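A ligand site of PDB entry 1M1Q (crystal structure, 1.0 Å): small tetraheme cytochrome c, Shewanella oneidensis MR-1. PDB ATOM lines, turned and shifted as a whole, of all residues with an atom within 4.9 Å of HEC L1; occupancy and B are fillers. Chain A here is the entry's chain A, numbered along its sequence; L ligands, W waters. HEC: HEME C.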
ATOM      1  N   SER A   6     -22.785   9.686 -12.051  1.00  0.00           N
ATOM      2  CA  SER A   6     -21.889  10.021 -13.206  1.00  0.00           C
ATOM      3  C   SER A   6     -20.689  10.832 -12.715  1.00  0.00           C
ATOM      4  O   SER A   6     -19.517  10.606 -13.091  1.00  0.00           O
ATOM      5  CB  SER A   6     -22.609  10.765 -14.238  1.00  0.00           C
ATOM      6  OG  SER A   6     -23.287  11.902 -13.702  1.00  0.00           O
ATOM      7  N   ASP A   7     -20.925  11.817 -11.848  1.00  0.00           N
ATOM      8  CA  ASP A   7     -19.879  12.686 -11.323  1.00  0.00           C
ATOM      9  C   ASP A   7     -18.931  11.905 -10.448  1.00  0.00           C
ATOM     10  O   ASP A   7     -17.707  12.157 -10.539  1.00  0.00           O
ATOM     11  CB  ASP A   7     -20.475  13.865 -10.606  1.00  0.00           C
ATOM     12  CG  ASP A   7     -21.177  14.828 -11.587  1.00  0.00           C
ATOM     13  OD1 ASP A   7     -20.703  15.057 -12.683  1.00  0.00           O
ATOM     14  OD2 ASP A   7     -22.201  15.441 -11.225  1.00  0.00           O
ATOM     15  N   HIS A   9     -18.106   8.746 -10.714  1.00  0.00           N
ATOM     16  CA  HIS A   9     -17.224   7.996 -11.615  1.00  0.00           C
ATOM     17  C   HIS A   9     -16.216   8.905 -12.345  1.00  0.00           C
ATOM     18  O   HIS A   9     -15.083   8.544 -12.515  1.00  0.00           O
ATOM     19  CB  HIS A   9     -17.995   7.199 -12.585  1.00  0.00           C
ATOM     20  CG  HIS A   9     -18.713   5.990 -12.092  1.00  0.00           C
ATOM     21  ND1 HIS A   9     -19.938   6.004 -11.462  1.00  0.00           N
ATOM     22  CD2 HIS A   9     -18.345   4.688 -12.122  1.00  0.00           C
ATOM     23  CE1 HIS A   9     -20.309   4.745 -11.145  1.00  0.00           C
ATOM     24  NE2 HIS A   9     -19.370   3.897 -11.554  1.00  0.00           N
ATOM     25  N   ALA A  10     -16.707  10.065 -12.784  1.00  0.00           N
ATOM     26  CA  ALA A  10     -15.789  10.944 -13.496  1.00  0.00           C
ATOM     27  C   ALA A  10     -14.620  11.406 -12.647  1.00  0.00           C
ATOM     28  O   ALA A  10     -13.594  11.760 -13.235  1.00  0.00           O
ATOM     29  CB  ALA A  10     -16.560  12.174 -14.005  1.00  0.00           C
ATOM     30  N   GLY A  14     -12.548  10.520 -15.432  1.00  0.00           N
ATOM     31  CA  GLY A  14     -13.073  11.478 -16.373  1.00  0.00           C
ATOM     32  C   GLY A  14     -14.395  10.975 -16.985  1.00  0.00           C
ATOM     33  O   GLY A  14     -14.855   9.882 -16.805  1.00  0.00           O
ATOM     34  N   CYS A  15     -14.948  11.885 -17.826  1.00  0.00           N
ATOM     35  CA  CYS A  15     -16.088  11.474 -18.615  1.00  0.00           C
ATOM     36  C   CYS A  15     -15.763  10.290 -19.514  1.00  0.00           C
ATOM     37  O   CYS A  15     -16.634   9.498 -19.845  1.00  0.00           O
ATOM     38  CB  CYS A  15     -16.574  12.670 -19.427  1.00  0.00           C
ATOM     39  SG  CYS A  15     -16.911  14.181 -18.562  1.00  0.00           S
ATOM     40  N   SER A  17     -14.211   7.722 -18.779  1.00  0.00           N
ATOM     41  CA  SER A  17     -14.344   6.429 -18.132  1.00  0.00           C
ATOM     42  C   SER A  17     -15.505   5.609 -18.747  1.00  0.00           C
ATOM     43  O   SER A  17     -15.453   4.399 -18.770  1.00  0.00           O
ATOM     44  CB  SER A  17     -14.598   6.608 -16.644  1.00  0.00           C
ATOM     45  OG  SER A  17     -14.422   5.370 -15.943  1.00  0.00           O
ATOM     46  N   CYS A  18     -16.562   6.334 -19.155  1.00  0.00           N
ATOM     47  CA  CYS A  18     -17.713   5.700 -19.746  1.00  0.00           C
ATOM     48  C   CYS A  18     -17.995   6.029 -21.190  1.00  0.00           C
ATOM     49  O   CYS A  18     -18.650   5.281 -21.873  1.00  0.00           O
ATOM     50  CB  CYS A  18     -18.991   6.025 -18.966  1.00  0.00           C
ATOM     51  SG  CYS A  18     -18.859   5.440 -17.257  1.00  0.00           S
ATOM     52  N   HIS A  19     -17.559   7.240 -21.653  1.00  0.00           N
ATOM     53  CA  HIS A  19     -17.915   7.743 -22.957  1.00  0.00           C
ATOM     54  C   HIS A  19     -16.683   7.949 -23.839  1.00  0.00           C
ATOM     55  O   HIS A  19     -15.677   8.565 -23.373  1.00  0.00           O
ATOM     56  CB  HIS A  19     -18.558   9.101 -22.872  1.00  0.00           C
ATOM     57  CG  HIS A  19     -19.837   9.168 -22.137  1.00  0.00           C
ATOM     58  ND1 HIS A  19     -20.953   8.479 -22.490  1.00  0.00           N
ATOM     59  CD2 HIS A  19     -20.229   9.926 -21.048  1.00  0.00           C
ATOM     60  CE1 HIS A  19     -21.934   8.833 -21.682  1.00  0.00           C
ATOM     61  NE2 HIS A  19     -21.550   9.699 -20.779  1.00  0.00           N
ATOM     62  N   GLY A  22     -15.280  11.345 -24.103  1.00  0.00           N
ATOM     63  CA  GLY A  22     -16.167  12.076 -23.186  1.00  0.00           C
ATOM     64  C   GLY A  22     -17.489  12.443 -23.738  1.00  0.00           C
ATOM     65  O   GLY A  22     -18.201  13.247 -23.141  1.00  0.00           O
ATOM     66  N   PRO A  24     -21.328  11.195 -25.390  1.00  0.00           N
ATOM     67  CA  PRO A  24     -22.203  10.033 -25.410  1.00  0.00           C
ATOM     68  C   PRO A  24     -22.406   9.492 -26.763  1.00  0.00           C
ATOM     69  O   PRO A  24     -22.522  10.209 -27.748  1.00  0.00           O
ATOM     70  CB  PRO A  24     -23.513  10.587 -24.805  1.00  0.00           C
ATOM     71  CG  PRO A  24     -23.473  12.070 -25.280  1.00  0.00           C
ATOM     72  CD  PRO A  24     -22.018  12.451 -25.052  1.00  0.00           C
ATOM     73  N   SER A  25     -22.562   8.138 -26.865  1.00  0.00           N
ATOM     74  CA  SER A  25     -22.979   7.472 -28.019  1.00  0.00           C
ATOM     75  C   SER A  25     -24.495   7.601 -28.179  1.00  0.00           C
ATOM     76  O   SER A  25     -25.208   7.900 -27.238  1.00  0.00           O
ATOM     77  CB  SER A  25     -22.699   5.971 -27.994  1.00  0.00           C
ATOM     78  OG  SER A  25     -23.504   5.289 -27.099  1.00  0.00           O
ATOM     79  N   ALA A  26     -24.995   7.343 -29.392  1.00  0.00           N
ATOM     80  CA  ALA A  26     -26.374   7.297 -29.634  1.00  0.00           C
ATOM     81  C   ALA A  26     -27.049   6.085 -29.073  1.00  0.00           C
ATOM     82  O   ALA A  26     -28.146   6.197 -28.569  1.00  0.00           O
ATOM     83  CB  ALA A  26     -26.565   7.367 -31.151  1.00  0.00           C
ATOM     84  N   ASP A  27     -26.417   4.932 -29.171  1.00  0.00           N
ATOM     85  CA  ASP A  27     -26.915   3.548 -28.978  1.00  0.00           C
ATOM     86  C   ASP A  27     -26.854   3.215 -27.435  1.00  0.00           C
ATOM     87  O   ASP A  27     -27.609   2.310 -26.995  1.00  0.00           O
ATOM     88  CB  ASP A  27     -26.180   2.529 -29.866  1.00  0.00           C
ATOM     89  CG  ASP A  27     -26.497   2.440 -31.345  1.00  0.00           C
ATOM     90  OD1 ASP A  27     -27.452   3.082 -31.700  1.00  0.00           O
ATOM     91  OD2 ASP A  27     -25.665   1.713 -31.992  1.00  0.00           O
ATOM     92  N   GLY A  28     -25.885   3.694 -26.695  1.00  0.00           N
ATOM     93  CA  GLY A  28     -25.572   3.278 -25.364  1.00  0.00           C
ATOM     94  C   GLY A  28     -24.774   1.977 -25.265  1.00  0.00           C
ATOM     95  O   GLY A  28     -24.441   1.547 -24.139  1.00  0.00           O
ATOM     96  N   GLU A  31     -21.159   2.547 -23.738  1.00  0.00           N
ATOM     97  CA  GLU A  31     -21.249   2.807 -22.313  1.00  0.00           C
ATOM     98  C   GLU A  31     -21.569   1.514 -21.551  1.00  0.00           C
ATOM     99  O   GLU A  31     -20.944   1.284 -20.501  1.00  0.00           O
ATOM    100  CB  GLU A  31     -22.344   3.867 -22.055  1.00  0.00           C
ATOM    101  CG  GLU A  31     -21.976   5.237 -22.564  1.00  0.00           C
ATOM    102  CD  GLU A  31     -22.069   5.530 -24.005  1.00  0.00           C
ATOM    103  OE1 GLU A  31     -22.603   4.692 -24.770  1.00  0.00           O
ATOM    104  OE2 GLU A  31     -21.598   6.634 -24.421  1.00  0.00           O
ATOM    105  N   ALA A  59     -27.915   0.978 -17.803  1.00  0.00           N
ATOM    106  CA  ALA A  59     -28.523   2.277 -17.835  1.00  0.00           C
ATOM    107  C   ALA A  59     -30.040   2.207 -17.885  1.00  0.00           C
ATOM    108  O   ALA A  59     -30.720   3.238 -17.669  1.00  0.00           O
ATOM    109  CB  ALA A  59     -28.023   3.066 -19.041  1.00  0.00           C
ATOM    110  N   VAL A  64     -27.409   7.248 -14.493  1.00  0.00           N
ATOM    111  CA  VAL A  64     -26.279   7.685 -13.690  1.00  0.00           C
ATOM    112  C   VAL A  64     -26.166   9.173 -13.621  1.00  0.00           C
ATOM    113  O   VAL A  64     -25.579   9.656 -12.636  1.00  0.00           O
ATOM    114  CB  VAL A  64     -24.915   7.076 -14.114  1.00  0.00           C
ATOM    115  CG1 VAL A  64     -25.000   5.509 -13.961  1.00  0.00           C
ATOM    116  CG2 VAL A  64     -24.520   7.458 -15.478  1.00  0.00           C
ATOM    117  N   HIS A  65     -26.699   9.914 -14.596  1.00  0.00           N
ATOM    118  CA  HIS A  65     -26.658  11.374 -14.474  1.00  0.00           C
ATOM    119  C   HIS A  65     -27.728  11.966 -13.592  1.00  0.00           C
ATOM    120  O   HIS A  65     -27.637  13.096 -13.158  1.00  0.00           O
ATOM    121  CB  HIS A  65     -26.764  11.976 -15.924  1.00  0.00           C
ATOM    122  CG  HIS A  65     -25.476  11.865 -16.649  1.00  0.00           C
ATOM    123  ND1 HIS A  65     -24.500  12.847 -16.554  1.00  0.00           N
ATOM    124  CD2 HIS A  65     -24.971  10.946 -17.511  1.00  0.00           C
ATOM    125  CE1 HIS A  65     -23.473  12.466 -17.339  1.00  0.00           C
ATOM    126  NE2 HIS A  65     -23.710  11.307 -17.907  1.00  0.00           N
HETATM  127 FE   HEC L   1     -22.609  10.478 -19.336  1.00  0.00          FE
HETATM  128  CHA HEC L   1     -25.532  10.041 -21.005  1.00  0.00           C
HETATM  129  CHB HEC L   1     -22.246  13.541 -20.714  1.00  0.00           C
HETATM  130  CHC HEC L   1     -19.828  11.025 -17.403  1.00  0.00           C
HETATM  131  CHD HEC L   1     -22.709   7.256 -18.328  1.00  0.00           C
HETATM  132  NA  HEC L   1     -23.667  11.550 -20.600  1.00  0.00           N
HETATM  133  C1A HEC L   1     -24.892  11.225 -21.143  1.00  0.00           C
HETATM  134  C2A HEC L   1     -25.365  12.295 -21.985  1.00  0.00           C
HETATM  135  C3A HEC L   1     -24.433  13.262 -21.934  1.00  0.00           C
HETATM  136  C4A HEC L   1     -23.366  12.774 -21.093  1.00  0.00           C
HETATM  137  CMA HEC L   1     -24.454  14.619 -22.627  1.00  0.00           C
HETATM  138  CAA HEC L   1     -26.697  12.354 -22.698  1.00  0.00           C
HETATM  139  CBA HEC L   1     -26.826  11.755 -23.972  1.00  0.00           C
HETATM  140  CGA HEC L   1     -28.072  12.062 -24.755  1.00  0.00           C
HETATM  141  O1A HEC L   1     -28.043  11.974 -26.001  1.00  0.00           O
HETATM  142  O2A HEC L   1     -29.005  12.628 -24.209  1.00  0.00           O
HETATM  143  NB  HEC L   1     -21.296  11.955 -19.115  1.00  0.00           N
HETATM  144  C1B HEC L   1     -21.293  13.175 -19.810  1.00  0.00           C
HETATM  145  C2B HEC L   1     -20.228  14.017 -19.328  1.00  0.00           C
HETATM  146  C3B HEC L   1     -19.548  13.343 -18.394  1.00  0.00           C
HETATM  147  C4B HEC L   1     -20.212  12.054 -18.256  1.00  0.00           C
HETATM  148  CMB HEC L   1     -19.951  15.432 -19.847  1.00  0.00           C
HETATM  149  CAB HEC L   1     -18.397  13.753 -17.566  1.00  0.00           C
HETATM  150  CBB HEC L   1     -18.630  14.911 -16.635  1.00  0.00           C
HETATM  151  NC  HEC L   1     -21.526   9.400 -18.084  1.00  0.00           N
HETATM  152  C1C HEC L   1     -20.411   9.760 -17.392  1.00  0.00           C
HETATM  153  C2C HEC L   1     -19.818   8.665 -16.670  1.00  0.00           C
HETATM  154  C3C HEC L   1     -20.601   7.578 -16.966  1.00  0.00           C
HETATM  155  C4C HEC L   1     -21.665   8.052 -17.842  1.00  0.00           C
HETATM  156  CMC HEC L   1     -18.533   8.738 -15.932  1.00  0.00           C
HETATM  157  CAC HEC L   1     -20.422   6.149 -16.560  1.00  0.00           C
HETATM  158  CBC HEC L   1     -20.449   5.890 -15.100  1.00  0.00           C
HETATM  159  ND  HEC L   1     -23.909   8.998 -19.562  1.00  0.00           N
HETATM  160  C1D HEC L   1     -23.707   7.647 -19.187  1.00  0.00           C
HETATM  161  C2D HEC L   1     -24.698   6.779 -19.799  1.00  0.00           C
HETATM  162  C3D HEC L   1     -25.509   7.519 -20.563  1.00  0.00           C
HETATM  163  C4D HEC L   1     -25.015   8.886 -20.362  1.00  0.00           C
HETATM  164  CMD HEC L   1     -24.876   5.253 -19.531  1.00  0.00           C
HETATM  165  CAD HEC L   1     -26.644   7.077 -21.467  1.00  0.00           C
HETATM  166  CBD HEC L   1     -26.288   6.272 -22.646  1.00  0.00           C
HETATM  167  CGD HEC L   1     -25.408   6.866 -23.804  1.00  0.00           C
HETATM  168  O1D HEC L   1     -24.615   7.546 -23.260  1.00  0.00           O
HETATM  169  O2D HEC L   1     -25.601   6.610 -24.889  1.00  0.00           O
HETATM  170 FE   HEC L   2     -19.437   1.916 -11.478  1.00  0.00          FE
HETATM  171  CHA HEC L   2     -19.619   2.340  -8.137  1.00  0.00           C
HETATM  172  CHB HEC L   2     -22.793   1.601 -11.635  1.00  0.00           C
HETATM  173  CHC HEC L   2     -19.278   2.271 -14.829  1.00  0.00           C
HETATM  174  CHD HEC L   2     -16.109   1.469 -11.305  1.00  0.00           C
HETATM  175  NA  HEC L   2     -20.913   1.978 -10.141  1.00  0.00           N
HETATM  176  C1A HEC L   2     -20.804   2.200  -8.788  1.00  0.00           C
HETATM  177  C2A HEC L   2     -22.103   2.189  -8.173  1.00  0.00           C
HETATM  178  C3A HEC L   2     -23.002   1.856  -9.147  1.00  0.00           C
HETATM  179  C4A HEC L   2     -22.224   1.763 -10.394  1.00  0.00           C
HETATM  180  CMA HEC L   2     -24.461   1.668  -9.035  1.00  0.00           C
HETATM  181  CAA HEC L   2     -22.351   2.292  -6.693  1.00  0.00           C
HETATM  182  CBA HEC L   2     -22.338   1.053  -5.925  1.00  0.00           C
HETATM  183  CGA HEC L   2     -22.469   1.184  -4.489  1.00  0.00           C
HETATM  184  O1A HEC L   2     -21.486   1.416  -3.757  1.00  0.00           O
HETATM  185  O2A HEC L   2     -23.567   1.043  -3.892  1.00  0.00           O
HETATM  186  NB  HEC L   2     -20.748   1.913 -12.931  1.00  0.00           N
HETATM  187  C1B HEC L   2     -22.117   1.684 -12.830  1.00  0.00           C
HETATM  188  C2B HEC L   2     -22.767   1.758 -14.139  1.00  0.00           C
HETATM  189  C3B HEC L   2     -21.755   2.046 -15.045  1.00  0.00           C
HETATM  190  C4B HEC L   2     -20.520   2.119 -14.278  1.00  0.00           C
HETATM  191  CMB HEC L   2     -24.224   1.558 -14.347  1.00  0.00           C
HETATM  192  CAB HEC L   2     -21.882   2.318 -16.477  1.00  0.00           C
HETATM  193  CBB HEC L   2     -22.886   3.429 -16.812  1.00  0.00           C
HETATM  194  NC  HEC L   2     -17.991   1.851 -12.821  1.00  0.00           N
HETATM  195  C1C HEC L   2     -18.078   2.099 -14.147  1.00  0.00           C
HETATM  196  C2C HEC L   2     -16.759   2.025 -14.800  1.00  0.00           C
HETATM  197  C3C HEC L   2     -15.888   1.690 -13.819  1.00  0.00           C
HETATM  198  C4C HEC L   2     -16.649   1.605 -12.566  1.00  0.00           C
HETATM  199  CMC HEC L   2     -16.511   2.274 -16.243  1.00  0.00           C
HETATM  200  CAC HEC L   2     -14.449   1.323 -13.940  1.00  0.00           C
HETATM  201  CBC HEC L   2     -13.566   2.377 -14.579  1.00  0.00           C
HETATM  202  ND  HEC L   2     -18.132   1.927 -10.023  1.00  0.00           N
HETATM  203  C1D HEC L   2     -16.779   1.687 -10.141  1.00  0.00           C
HETATM  204  C2D HEC L   2     -16.136   1.746  -8.828  1.00  0.00           C
HETATM  205  C3D HEC L   2     -17.145   2.070  -7.945  1.00  0.00           C
HETATM  206  C4D HEC L   2     -18.363   2.170  -8.668  1.00  0.00           C
HETATM  207  CMD HEC L   2     -14.702   1.501  -8.556  1.00  0.00           C
HETATM  208  CAD HEC L   2     -16.982   2.270  -6.460  1.00  0.00           C
HETATM  209  CBD HEC L   2     -17.223   1.051  -5.622  1.00  0.00           C
HETATM  210  CGD HEC L   2     -18.654   0.904  -5.197  1.00  0.00           C
HETATM  211  O1D HEC L   2     -19.186   2.000  -4.691  1.00  0.00           O
HETATM  212  O2D HEC L   2     -19.175  -0.211  -5.451  1.00  0.00           O
HETATM  213  O   HOH W   1     -30.171  13.394 -21.628  1.00  0.00           O
HETATM  214  O   HOH W   2     -30.499  13.008 -26.776  1.00  0.00           O
HETATM  215  O   HOH W   3     -27.110   5.875 -17.126  1.00  0.00           O
HETATM  216  O   HOH W   4     -27.414   9.445 -26.616  1.00  0.00           O
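Water W4 lies within hydrogen-bond range of an oxygen (O1A) of HEC L1 (2.7 Å) and the backbone carbonyl oxygen (O) of Ser 25 (2.8 Å).
A ring nitrogen (ND1) of His 19 is in hydrogen-bond range of the side-chain carboxylate of Glu 31 (2.7 Å). ND1 of His 65 is in hydrogen-bond range of OG of Ser 6 (3.2 Å). The side-chain hydroxyl (OG) of Ser 25 is in hydrogen-bond range of the side-chain carboxylate (OE1) of Glu 31. OG of Ser 25 is in hydrogen-bond range of N of Gly 28 (2.9 Å). The backbone carbonyl oxygen (O) of Val 64 is in hydrogen-bond range of the backbone NH (N) of Ser 6, 2.9 Å away.
A carbon (CAB) of HEC L1 is covalently linked to the side-chain sulfur (SG) of Cys 15 (1.8 Å). SG of Cys 18 is bonded to CAC of HEC L1 (1.9 Å). An iron atom (FE) of HEC L1 is bound by a ring nitrogen (NE2) of His 19 (2.0 Å). A ring nitrogen (NE2) of His 65 is bound to an iron atom (FE) of HEC L1. O of Ser 25 sits close to O2D of HEC L1. OG of Ser 25 sits at hydrogen-bond distance from O2D of HEC L1 (3.3 Å). An oxygen (O2D) of HEC L1 sits close to the backbone NH (N) of Gly 28. An iron atom (FE) of HEC L2 is bound by a ring nitrogen (NE2) of His 9.
The side-chain carboxylate of Glu 31 sits close to an oxygen (O1D) of HEC L1, 3.4 Å away. Ser 6 touches HEC L1 (O to CMC, 3.5 Å). His 9 touches HEC L1. Ala 10 touches HEC L1. Gly 14 touches HEC L1 (O to CMC, 3.9 Å). CB of Pro 24 touches O1D of HEC L1, at 3.6 Å. CB of Ala 59 touches CMD of HEC L1, 3.9 Å away. CG2 of Val 64 touches CHD of HEC L1, at 3.4 Å. Hydrophobic or aromatic side chains within 4 Å of HEC L1: His 9, His 19, Pro 24, Ala 59, Val 64 and His 65.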
